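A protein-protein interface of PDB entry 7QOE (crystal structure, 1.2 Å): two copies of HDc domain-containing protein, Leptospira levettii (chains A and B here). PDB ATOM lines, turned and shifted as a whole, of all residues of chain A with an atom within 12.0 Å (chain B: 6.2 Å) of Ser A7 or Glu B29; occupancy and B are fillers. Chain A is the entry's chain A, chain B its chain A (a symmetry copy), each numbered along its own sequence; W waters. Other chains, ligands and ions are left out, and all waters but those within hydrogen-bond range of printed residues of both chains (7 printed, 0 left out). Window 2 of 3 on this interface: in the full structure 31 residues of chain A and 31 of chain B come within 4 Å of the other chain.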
ATOM      1  N   GLN A   4      30.104  13.884 -10.027  1.00  0.00           N
ATOM      2  CA  GLN A   4      29.107  14.421 -10.952  1.00  0.00           C
ATOM      3  C   GLN A   4      29.765  14.690 -12.300  1.00  0.00           C
ATOM      4  O   GLN A   4      29.413  15.632 -13.016  1.00  0.00           O
ATOM      5  CB  GLN A   4      28.489  15.689 -10.377  1.00  0.00           C
ATOM      6  CG  GLN A   4      29.497  16.658  -9.781  1.00  0.00           C
ATOM      7  CD  GLN A   4      28.929  18.052  -9.605  1.00  0.00           C
ATOM      8  OE1 GLN A   4      29.644  19.047  -9.746  1.00  0.00           O
ATOM      9  NE2 GLN A   4      27.643  18.134  -9.267  1.00  0.00           N
ATOM     10  N   VAL A   5      30.744  13.848 -12.633  1.00  0.00           N
ATOM     11  CA  VAL A   5      31.403  13.942 -13.927  1.00  0.00           C
ATOM     12  C   VAL A   5      30.380  13.783 -15.043  1.00  0.00           C
ATOM     13  O   VAL A   5      29.472  12.947 -14.967  1.00  0.00           O
ATOM     14  CB  VAL A   5      32.486  12.851 -14.016  1.00  0.00           C
ATOM     15  CG1 VAL A   5      32.967  12.672 -15.453  1.00  0.00           C
ATOM     16  CG2 VAL A   5      33.643  13.177 -13.080  1.00  0.00           C
ATOM     17  N   ASP A   6      30.516  14.592 -16.089  1.00  0.00           N
ATOM     18  CA  ASP A   6      29.728  14.401 -17.304  1.00  0.00           C
ATOM     19  C   ASP A   6      30.529  13.512 -18.247  1.00  0.00           C
ATOM     20  O   ASP A   6      31.578  13.923 -18.757  1.00  0.00           O
ATOM     21  CB  ASP A   6      29.398  15.734 -17.964  1.00  0.00           C
ATOM     22  CG  ASP A   6      28.362  16.524 -17.190  1.00  0.00           C
ATOM     23  OD1 ASP A   6      27.473  15.901 -16.571  1.00  0.00           O
ATOM     24  OD2 ASP A   6      28.441  17.769 -17.200  1.00  0.00           O
ATOM     25  N   SER A   7      30.043  12.298 -18.481  1.00  0.00           N
ATOM     26  CA  SER A   7      30.739  11.400 -19.390  1.00  0.00           C
ATOM     27  C   SER A   7      30.709  11.950 -20.816  1.00  0.00           C
ATOM     28  O   SER A   7      29.895  12.811 -21.167  1.00  0.00           O
ATOM     29  CB  SER A   7      30.095  10.015 -19.381  1.00  0.00           C
ATOM     30  OG  SER A   7      28.778  10.066 -19.895  1.00  0.00           O
ATOM     31  N   TYR A   8      31.608  11.426 -21.646  1.00  0.00           N
ATOM     32  CA  TYR A   8      31.752  11.905 -23.017  1.00  0.00           C
ATOM     33  C   TYR A   8      30.684  11.279 -23.911  1.00  0.00           C
ATOM     34  O   TYR A   8      30.625  10.051 -24.055  1.00  0.00           O
ATOM     35  CB  TYR A   8      33.149  11.573 -23.539  1.00  0.00           C
ATOM     36  CG  TYR A   8      33.391  11.980 -24.982  1.00  0.00           C
ATOM     37  CD1 TYR A   8      33.473  13.317 -25.338  1.00  0.00           C
ATOM     38  CD2 TYR A   8      33.546  11.025 -25.979  1.00  0.00           C
ATOM     39  CE1 TYR A   8      33.696  13.696 -26.641  1.00  0.00           C
ATOM     40  CE2 TYR A   8      33.765  11.394 -27.285  1.00  0.00           C
ATOM     41  CZ  TYR A   8      33.841  12.733 -27.610  1.00  0.00           C
ATOM     42  OH  TYR A   8      34.068  13.109 -28.912  1.00  0.00           O
ATOM     43  N   ARG A   9      29.856  12.132 -24.509  1.00  0.00           N
ATOM     44  CA  ARG A   9      28.852  11.723 -25.484  1.00  0.00           C
ATOM     45  C   ARG A   9      28.069  10.479 -25.058  1.00  0.00           C
ATOM     46  O   ARG A   9      28.036   9.476 -25.786  1.00  0.00           O
ATOM     47  CB  ARG A   9      29.471  11.518 -26.859  1.00  0.00           C
ATOM     48  CG  ARG A   9      30.031  12.775 -27.513  1.00  0.00           C
ATOM     49  CD  ARG A   9      30.604  12.465 -28.900  1.00  0.00           C
ATOM     50  NE  ARG A   9      30.805  13.668 -29.698  1.00  0.00           N
ATOM     51  CZ  ARG A   9      29.868  14.256 -30.428  1.00  0.00           C
ATOM     52  NH1 ARG A   9      28.637  13.776 -30.488  1.00  0.00           N
ATOM     53  NH2 ARG A   9      30.173  15.356 -31.110  1.00  0.00           N
ATOM     54  N   PRO A  10      27.440  10.500 -23.884  1.00  0.00           N
ATOM     55  CA  PRO A  10      26.544   9.397 -23.519  1.00  0.00           C
ATOM     56  C   PRO A  10      25.284   9.445 -24.363  1.00  0.00           C
ATOM     57  O   PRO A  10      24.849  10.507 -24.818  1.00  0.00           O
ATOM     58  CB  PRO A  10      26.220   9.667 -22.046  1.00  0.00           C
ATOM     59  CG  PRO A  10      26.303  11.156 -21.931  1.00  0.00           C
ATOM     60  CD  PRO A  10      27.439  11.568 -22.865  1.00  0.00           C
ATOM     61  N   LYS A  11      24.679   8.275 -24.564  1.00  0.00           N
ATOM     62  CA  LYS A  11      23.467   8.243 -25.372  1.00  0.00           C
ATOM     63  C   LYS A  11      22.366   9.086 -24.730  1.00  0.00           C
ATOM     64  O   LYS A  11      21.697   9.864 -25.415  1.00  0.00           O
ATOM     65  CB  LYS A  11      23.000   6.809 -25.602  1.00  0.00           C
ATOM     66  CG  LYS A  11      21.781   6.711 -26.516  1.00  0.00           C
ATOM     67  CD  LYS A  11      22.102   6.099 -27.869  1.00  0.00           C
ATOM     68  CE  LYS A  11      20.833   5.644 -28.585  1.00  0.00           C
ATOM     69  NZ  LYS A  11      20.439   4.253 -28.213  1.00  0.00           N
ATOM     70  N   LEU A  12      22.173   8.956 -23.411  1.00  0.00           N
ATOM     71  CA  LEU A  12      21.150   9.702 -22.675  1.00  0.00           C
ATOM     72  C   LEU A  12      21.884  10.667 -21.748  1.00  0.00           C
ATOM     73  O   LEU A  12      22.358  10.274 -20.675  1.00  0.00           O
ATOM     74  CB  LEU A  12      20.244   8.744 -21.918  1.00  0.00           C
ATOM     75  CG  LEU A  12      19.454   7.797 -22.822  1.00  0.00           C
ATOM     76  CD1 LEU A  12      18.570   6.872 -21.979  1.00  0.00           C
ATOM     77  CD2 LEU A  12      18.610   8.539 -23.843  1.00  0.00           C
ATOM     78  N   GLY A  13      21.972  11.927 -22.175  1.00  0.00           N
ATOM     79  CA  GLY A  13      22.816  12.913 -21.531  1.00  0.00           C
ATOM     80  C   GLY A  13      22.089  14.132 -20.994  1.00  0.00           C
ATOM     81  O   GLY A  13      20.973  14.008 -20.483  1.00  0.00           O
ATOM     82  N   LYS A  14      22.710  15.313 -21.127  1.00  0.00           N
ATOM     83  CA  LYS A  14      22.221  16.507 -20.443  1.00  0.00           C
ATOM     84  C   LYS A  14      20.773  16.828 -20.795  1.00  0.00           C
ATOM     85  O   LYS A  14      19.982  17.185 -19.911  1.00  0.00           O
ATOM     86  CB  LYS A  14      23.121  17.702 -20.777  1.00  0.00           C
ATOM     87  CG  LYS A  14      22.835  18.947 -19.950  1.00  0.00           C
ATOM     88  CD  LYS A  14      24.105  19.709 -19.601  1.00  0.00           C
ATOM     89  CE  LYS A  14      24.891  19.025 -18.496  1.00  0.00           C
ATOM     90  NZ  LYS A  14      26.051  19.848 -18.055  1.00  0.00           N
ATOM     91  N   LYS A  15      20.411  16.738 -22.077  1.00  0.00           N
ATOM     92  CA  LYS A  15      19.046  17.090 -22.469  1.00  0.00           C
ATOM     93  C   LYS A  15      18.040  16.091 -21.908  1.00  0.00           C
ATOM     94  O   LYS A  15      16.938  16.475 -21.503  1.00  0.00           O
ATOM     95  CB  LYS A  15      18.924  17.188 -23.991  1.00  0.00           C
ATOM     96  CG  LYS A  15      19.743  18.291 -24.651  1.00  0.00           C
ATOM     97  CD  LYS A  15      19.711  19.601 -23.895  1.00  0.00           C
ATOM     98  CE  LYS A  15      18.354  20.285 -23.982  1.00  0.00           C
ATOM     99  NZ  LYS A  15      18.507  21.769 -23.738  1.00  0.00           N
ATOM    100  N   PHE A  16      18.386  14.800 -21.916  1.00  0.00           N
ATOM    101  CA  PHE A  16      17.527  13.802 -21.286  1.00  0.00           C
ATOM    102  C   PHE A  16      17.342  14.107 -19.804  1.00  0.00           C
ATOM    103  O   PHE A  16      16.228  13.993 -19.271  1.00  0.00           O
ATOM    104  CB  PHE A  16      18.148  12.427 -21.524  1.00  0.00           C
ATOM    105  CG  PHE A  16      17.642  11.339 -20.610  1.00  0.00           C
ATOM    106  CD1 PHE A  16      16.393  10.768 -20.807  1.00  0.00           C
ATOM    107  CD2 PHE A  16      18.444  10.861 -19.591  1.00  0.00           C
ATOM    108  CE1 PHE A  16      15.962   9.741 -19.971  1.00  0.00           C
ATOM    109  CE2 PHE A  16      18.015   9.850 -18.768  1.00  0.00           C
ATOM    110  CZ  PHE A  16      16.775   9.288 -18.966  1.00  0.00           C
ATOM    111  N   ASN A  17      18.420  14.505 -19.117  1.00  0.00           N
ATOM    112  CA  ASN A  17      18.312  14.811 -17.686  1.00  0.00           C
ATOM    113  C   ASN A  17      17.439  16.034 -17.460  1.00  0.00           C
ATOM    114  O   ASN A  17      16.661  16.085 -16.499  1.00  0.00           O
ATOM    115  CB  ASN A  17      19.715  14.990 -17.123  1.00  0.00           C
ATOM    116  CG  ASN A  17      20.521  13.709 -17.190  1.00  0.00           C
ATOM    117  OD1 ASN A  17      19.951  12.625 -17.327  1.00  0.00           O
ATOM    118  ND2 ASN A  17      21.836  13.818 -17.074  1.00  0.00           N
ATOM    119  N   GLU A  57      17.945   9.429 -27.958  1.00  0.00           N
ATOM    120  CA  GLU A  57      17.656  10.420 -26.920  1.00  0.00           C
ATOM    121  C   GLU A  57      16.396  11.207 -27.258  1.00  0.00           C
ATOM    122  O   GLU A  57      15.550  11.447 -26.388  1.00  0.00           O
ATOM    123  CB  GLU A  57      18.847  11.359 -26.701  1.00  0.00           C
ATOM    124  CG  GLU A  57      18.700  12.203 -25.437  1.00  0.00           C
ATOM    125  CD  GLU A  57      19.772  13.273 -25.248  1.00  0.00           C
ATOM    126  OE1 GLU A  57      20.092  14.005 -26.205  1.00  0.00           O
ATOM    127  OE2 GLU A  57      20.333  13.350 -24.136  1.00  0.00           O
ATOM    128  N   SER B  24      21.045   9.373 -13.225  1.00  0.00           N
ATOM    129  CA  SER B  24      21.364   9.351 -14.646  1.00  0.00           C
ATOM    130  C   SER B  24      22.805   9.767 -14.897  1.00  0.00           C
ATOM    131  O   SER B  24      23.483   9.182 -15.753  1.00  0.00           O
ATOM    132  CB  SER B  24      20.410  10.276 -15.377  1.00  0.00           C
ATOM    133  OG  SER B  24      20.650  10.173 -16.764  1.00  0.00           O
ATOM    134  N   GLU B  25      23.289  10.780 -14.177  1.00  0.00           N
ATOM    135  CA  GLU B  25      24.681  11.188 -14.324  1.00  0.00           C
ATOM    136  C   GLU B  25      25.623  10.101 -13.823  1.00  0.00           C
ATOM    137  O   GLU B  25      26.621   9.774 -14.480  1.00  0.00           O
ATOM    138  CB  GLU B  25      24.914  12.515 -13.604  1.00  0.00           C
ATOM    139  CG  GLU B  25      24.244  13.702 -14.290  1.00  0.00           C
ATOM    140  CD  GLU B  25      24.435  15.012 -13.563  1.00  0.00           C
ATOM    141  OE1 GLU B  25      24.899  14.986 -12.405  1.00  0.00           O
ATOM    142  OE2 GLU B  25      24.121  16.072 -14.154  1.00  0.00           O
ATOM    143  N   LEU B  26      25.311   9.508 -12.677  1.00  0.00           N
ATOM    144  CA  LEU B  26      26.206   8.520 -12.085  1.00  0.00           C
ATOM    145  C   LEU B  26      26.326   7.275 -12.958  1.00  0.00           C
ATOM    146  O   LEU B  26      27.422   6.718 -13.096  1.00  0.00           O
ATOM    147  CB  LEU B  26      25.679   8.166 -10.697  1.00  0.00           C
ATOM    148  CG  LEU B  26      26.579   7.335  -9.798  1.00  0.00           C
ATOM    149  CD1 LEU B  26      27.752   8.164  -9.314  1.00  0.00           C
ATOM    150  CD2 LEU B  26      25.773   6.825  -8.613  1.00  0.00           C
ATOM    151  N   HIS B  27      25.223   6.848 -13.578  1.00  0.00           N
ATOM    152  CA  HIS B  27      25.165   5.630 -14.373  1.00  0.00           C
ATOM    153  C   HIS B  27      25.196   5.901 -15.880  1.00  0.00           C
ATOM    154  O   HIS B  27      24.882   5.001 -16.669  1.00  0.00           O
ATOM    155  CB  HIS B  27      23.914   4.797 -14.017  1.00  0.00           C
ATOM    156  CG  HIS B  27      23.884   4.306 -12.595  1.00  0.00           C
ATOM    157  ND1 HIS B  27      24.271   3.029 -12.247  1.00  0.00           N
ATOM    158  CD2 HIS B  27      23.433   4.878 -11.453  1.00  0.00           C
ATOM    159  CE1 HIS B  27      24.128   2.859 -10.943  1.00  0.00           C
ATOM    160  NE2 HIS B  27      23.604   3.963 -10.439  1.00  0.00           N
ATOM    161  N   ALA B  28      25.608   7.108 -16.287  1.00  0.00           N
ATOM    162  CA  ALA B  28      25.483   7.524 -17.684  1.00  0.00           C
ATOM    163  C   ALA B  28      26.186   6.581 -18.649  1.00  0.00           C
ATOM    164  O   ALA B  28      25.720   6.391 -19.779  1.00  0.00           O
ATOM    165  CB  ALA B  28      26.066   8.926 -17.854  1.00  0.00           C
ATOM    166  N   GLU B  29      27.326   6.030 -18.249  1.00  0.00           N
ATOM    167  CA  GLU B  29      28.139   5.201 -19.126  1.00  0.00           C
ATOM    168  C   GLU B  29      27.890   3.721 -18.943  1.00  0.00           C
ATOM    169  O   GLU B  29      28.476   2.912 -19.670  1.00  0.00           O
ATOM    170  CB  GLU B  29      29.616   5.451 -18.876  1.00  0.00           C
ATOM    171  CG  GLU B  29      30.059   6.832 -19.144  1.00  0.00           C
ATOM    172  CD  GLU B  29      31.499   6.853 -19.547  1.00  0.00           C
ATOM    173  OE1 GLU B  29      31.780   7.290 -20.683  1.00  0.00           O
ATOM    174  OE2 GLU B  29      32.345   6.407 -18.739  1.00  0.00           O
ATOM    175  N   GLN B  30      27.075   3.345 -17.964  1.00  0.00           N
ATOM    176  CA  GLN B  30      26.804   1.947 -17.689  1.00  0.00           C
ATOM    177  C   GLN B  30      25.724   1.450 -18.639  1.00  0.00           C
ATOM    178  O   GLN B  30      24.800   2.183 -19.004  1.00  0.00           O
ATOM    179  CB  GLN B  30      26.372   1.786 -16.229  1.00  0.00           C
ATOM    180  CG  GLN B  30      26.206   0.338 -15.777  1.00  0.00           C
ATOM    181  CD  GLN B  30      25.876   0.230 -14.307  1.00  0.00           C
ATOM    182  OE1 GLN B  30      25.959   1.210 -13.563  1.00  0.00           O
ATOM    183  NE2 GLN B  30      25.472  -0.967 -13.874  1.00  0.00           N
ATOM    184  N   ARG B  31      25.846   0.189 -19.043  1.00  0.00           N
ATOM    185  CA  ARG B  31      24.890  -0.442 -19.938  1.00  0.00           C
ATOM    186  C   ARG B  31      24.321  -1.687 -19.277  1.00  0.00           C
ATOM    187  O   ARG B  31      24.993  -2.351 -18.479  1.00  0.00           O
ATOM    188  CB  ARG B  31      25.558  -0.842 -21.266  1.00  0.00           C
ATOM    189  CG  ARG B  31      26.069   0.341 -22.095  1.00  0.00           C
ATOM    190  CD  ARG B  31      27.101  -0.062 -23.158  1.00  0.00           C
ATOM    191  NE  ARG B  31      28.176  -0.883 -22.609  1.00  0.00           N
ATOM    192  CZ  ARG B  31      29.185  -0.418 -21.885  1.00  0.00           C
ATOM    193  NH1 ARG B  31      29.291   0.867 -21.592  1.00  0.00           N
ATOM    194  NH2 ARG B  31      30.109  -1.265 -21.441  1.00  0.00           N
ATOM    195  N   GLN B  72      28.731   1.949  -8.837  1.00  0.00           N
ATOM    196  CA  GLN B  72      29.201   3.293  -9.163  1.00  0.00           C
ATOM    197  C   GLN B  72      29.880   3.989  -7.991  1.00  0.00           C
ATOM    198  O   GLN B  72      29.701   5.194  -7.783  1.00  0.00           O
ATOM    199  CB  GLN B  72      28.081   4.162  -9.749  1.00  0.00           C
ATOM    200  CG  GLN B  72      27.525   3.659 -11.069  1.00  0.00           C
ATOM    201  CD  GLN B  72      28.538   3.730 -12.204  1.00  0.00           C
ATOM    202  OE1 GLN B  72      29.558   4.410 -12.108  1.00  0.00           O
ATOM    203  NE2 GLN B  72      28.261   3.009 -13.279  1.00  0.00           N
HETATM  204  O   HOH W   1      29.679   8.136 -22.160  1.00  0.00           O
HETATM  205  O   HOH W   2      22.005   7.993 -18.270  1.00  0.00           O
HETATM  206  O   HOH W   3      23.513   7.342 -21.346  1.00  0.00           O
HETATM  207  O   HOH W   4      22.989  16.310 -16.461  1.00  0.00           O
HETATM  208  O   HOH W   5      23.283  11.197 -18.106  1.00  0.00           O
HETATM  209  O   HOH W   6      33.284   9.412 -20.747  1.00  0.00           O
HETATM  210  O   HOH W   7      27.819  11.651 -16.400  1.00  0.00           O
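The side-chain hydroxyl (OG) of Ser B24 lies within hydrogen-bond range of the side-chain amide oxygen (OD1) of Asn A17, at 2.6 Å.
The backbone NH (N) of Phe A16 sits at hydrogen-bond distance from the side-chain carboxylate (OE2) of Glu A57 (3.3 Å).
NH1 of Arg B31 lies within hydrogen-bond range of O of Glu B29, 2.9 Å away.
Among the printed residues, merely in contact across the chains: Ser A7 with Ala B28 (3.6 Å), Ser A7 with Glu B29 (3.2 Å), Phe A16 with Ser B24 (3.3 Å) and Asn A17 with Glu B25 (3.7 Å).
Of chain B, only Ala B28 (3.6 Å) and Glu B29 (3.2 Å) come within 4 Å of Ser A7.
Of chain A, only Ser A7 (3.2 Å) comes within 4 Å of Glu B29.
No residue of chain A comes within 4 Å of Gln B30.
Printed residues of chain A within 4 Å of Glu B25: Asn A17.
Printed residues of chain B within 4 Å of Phe A16: Ser B24.
Of the 9 printed residues of chain B, 4 touch a printed residue of chain A.
Of the 15 printed residues of chain A, 3 touch a printed residue of chain B.
Among the printed residues, 5 pairs touch across the chains.
Among the printed residues, no Asp or Glu carboxylate lies within 4 Å of a Lys or Arg side-chain nitrogen of the other chain.
No position is printed for both chains.
Of the 5 pairs that touch across the chains among the printed residues, none has its exchanged pair printed and touching as well.
Water W7 lies within hydrogen-bond range of O of Val A5, O of Glu B25 and N of Ser A7.
Water W4 lies within hydrogen-bond range of the side-chain carboxylate of Glu B25 (2.6 Å) and the side-chain amide nitrogen of Asn A17 (2.8 Å).
Water W6 lies within hydrogen-bond range of the side-chain carboxylate of Glu B29 and the backbone NH of Tyr A8.
Water W1 lies within hydrogen-bond range of OE1 of Glu B29 (2.7 Å), O of Tyr A8 (2.9 Å) and OG of Ser A7 (3.1 Å).
Water W3 lies within hydrogen-bond range of O of Ala B28 (2.9 Å) and N of Leu A12 (2.9 Å).
Water W5 lies within hydrogen-bond range of O of Leu A12, O of Ser B24 and ND2 of Asn A17.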
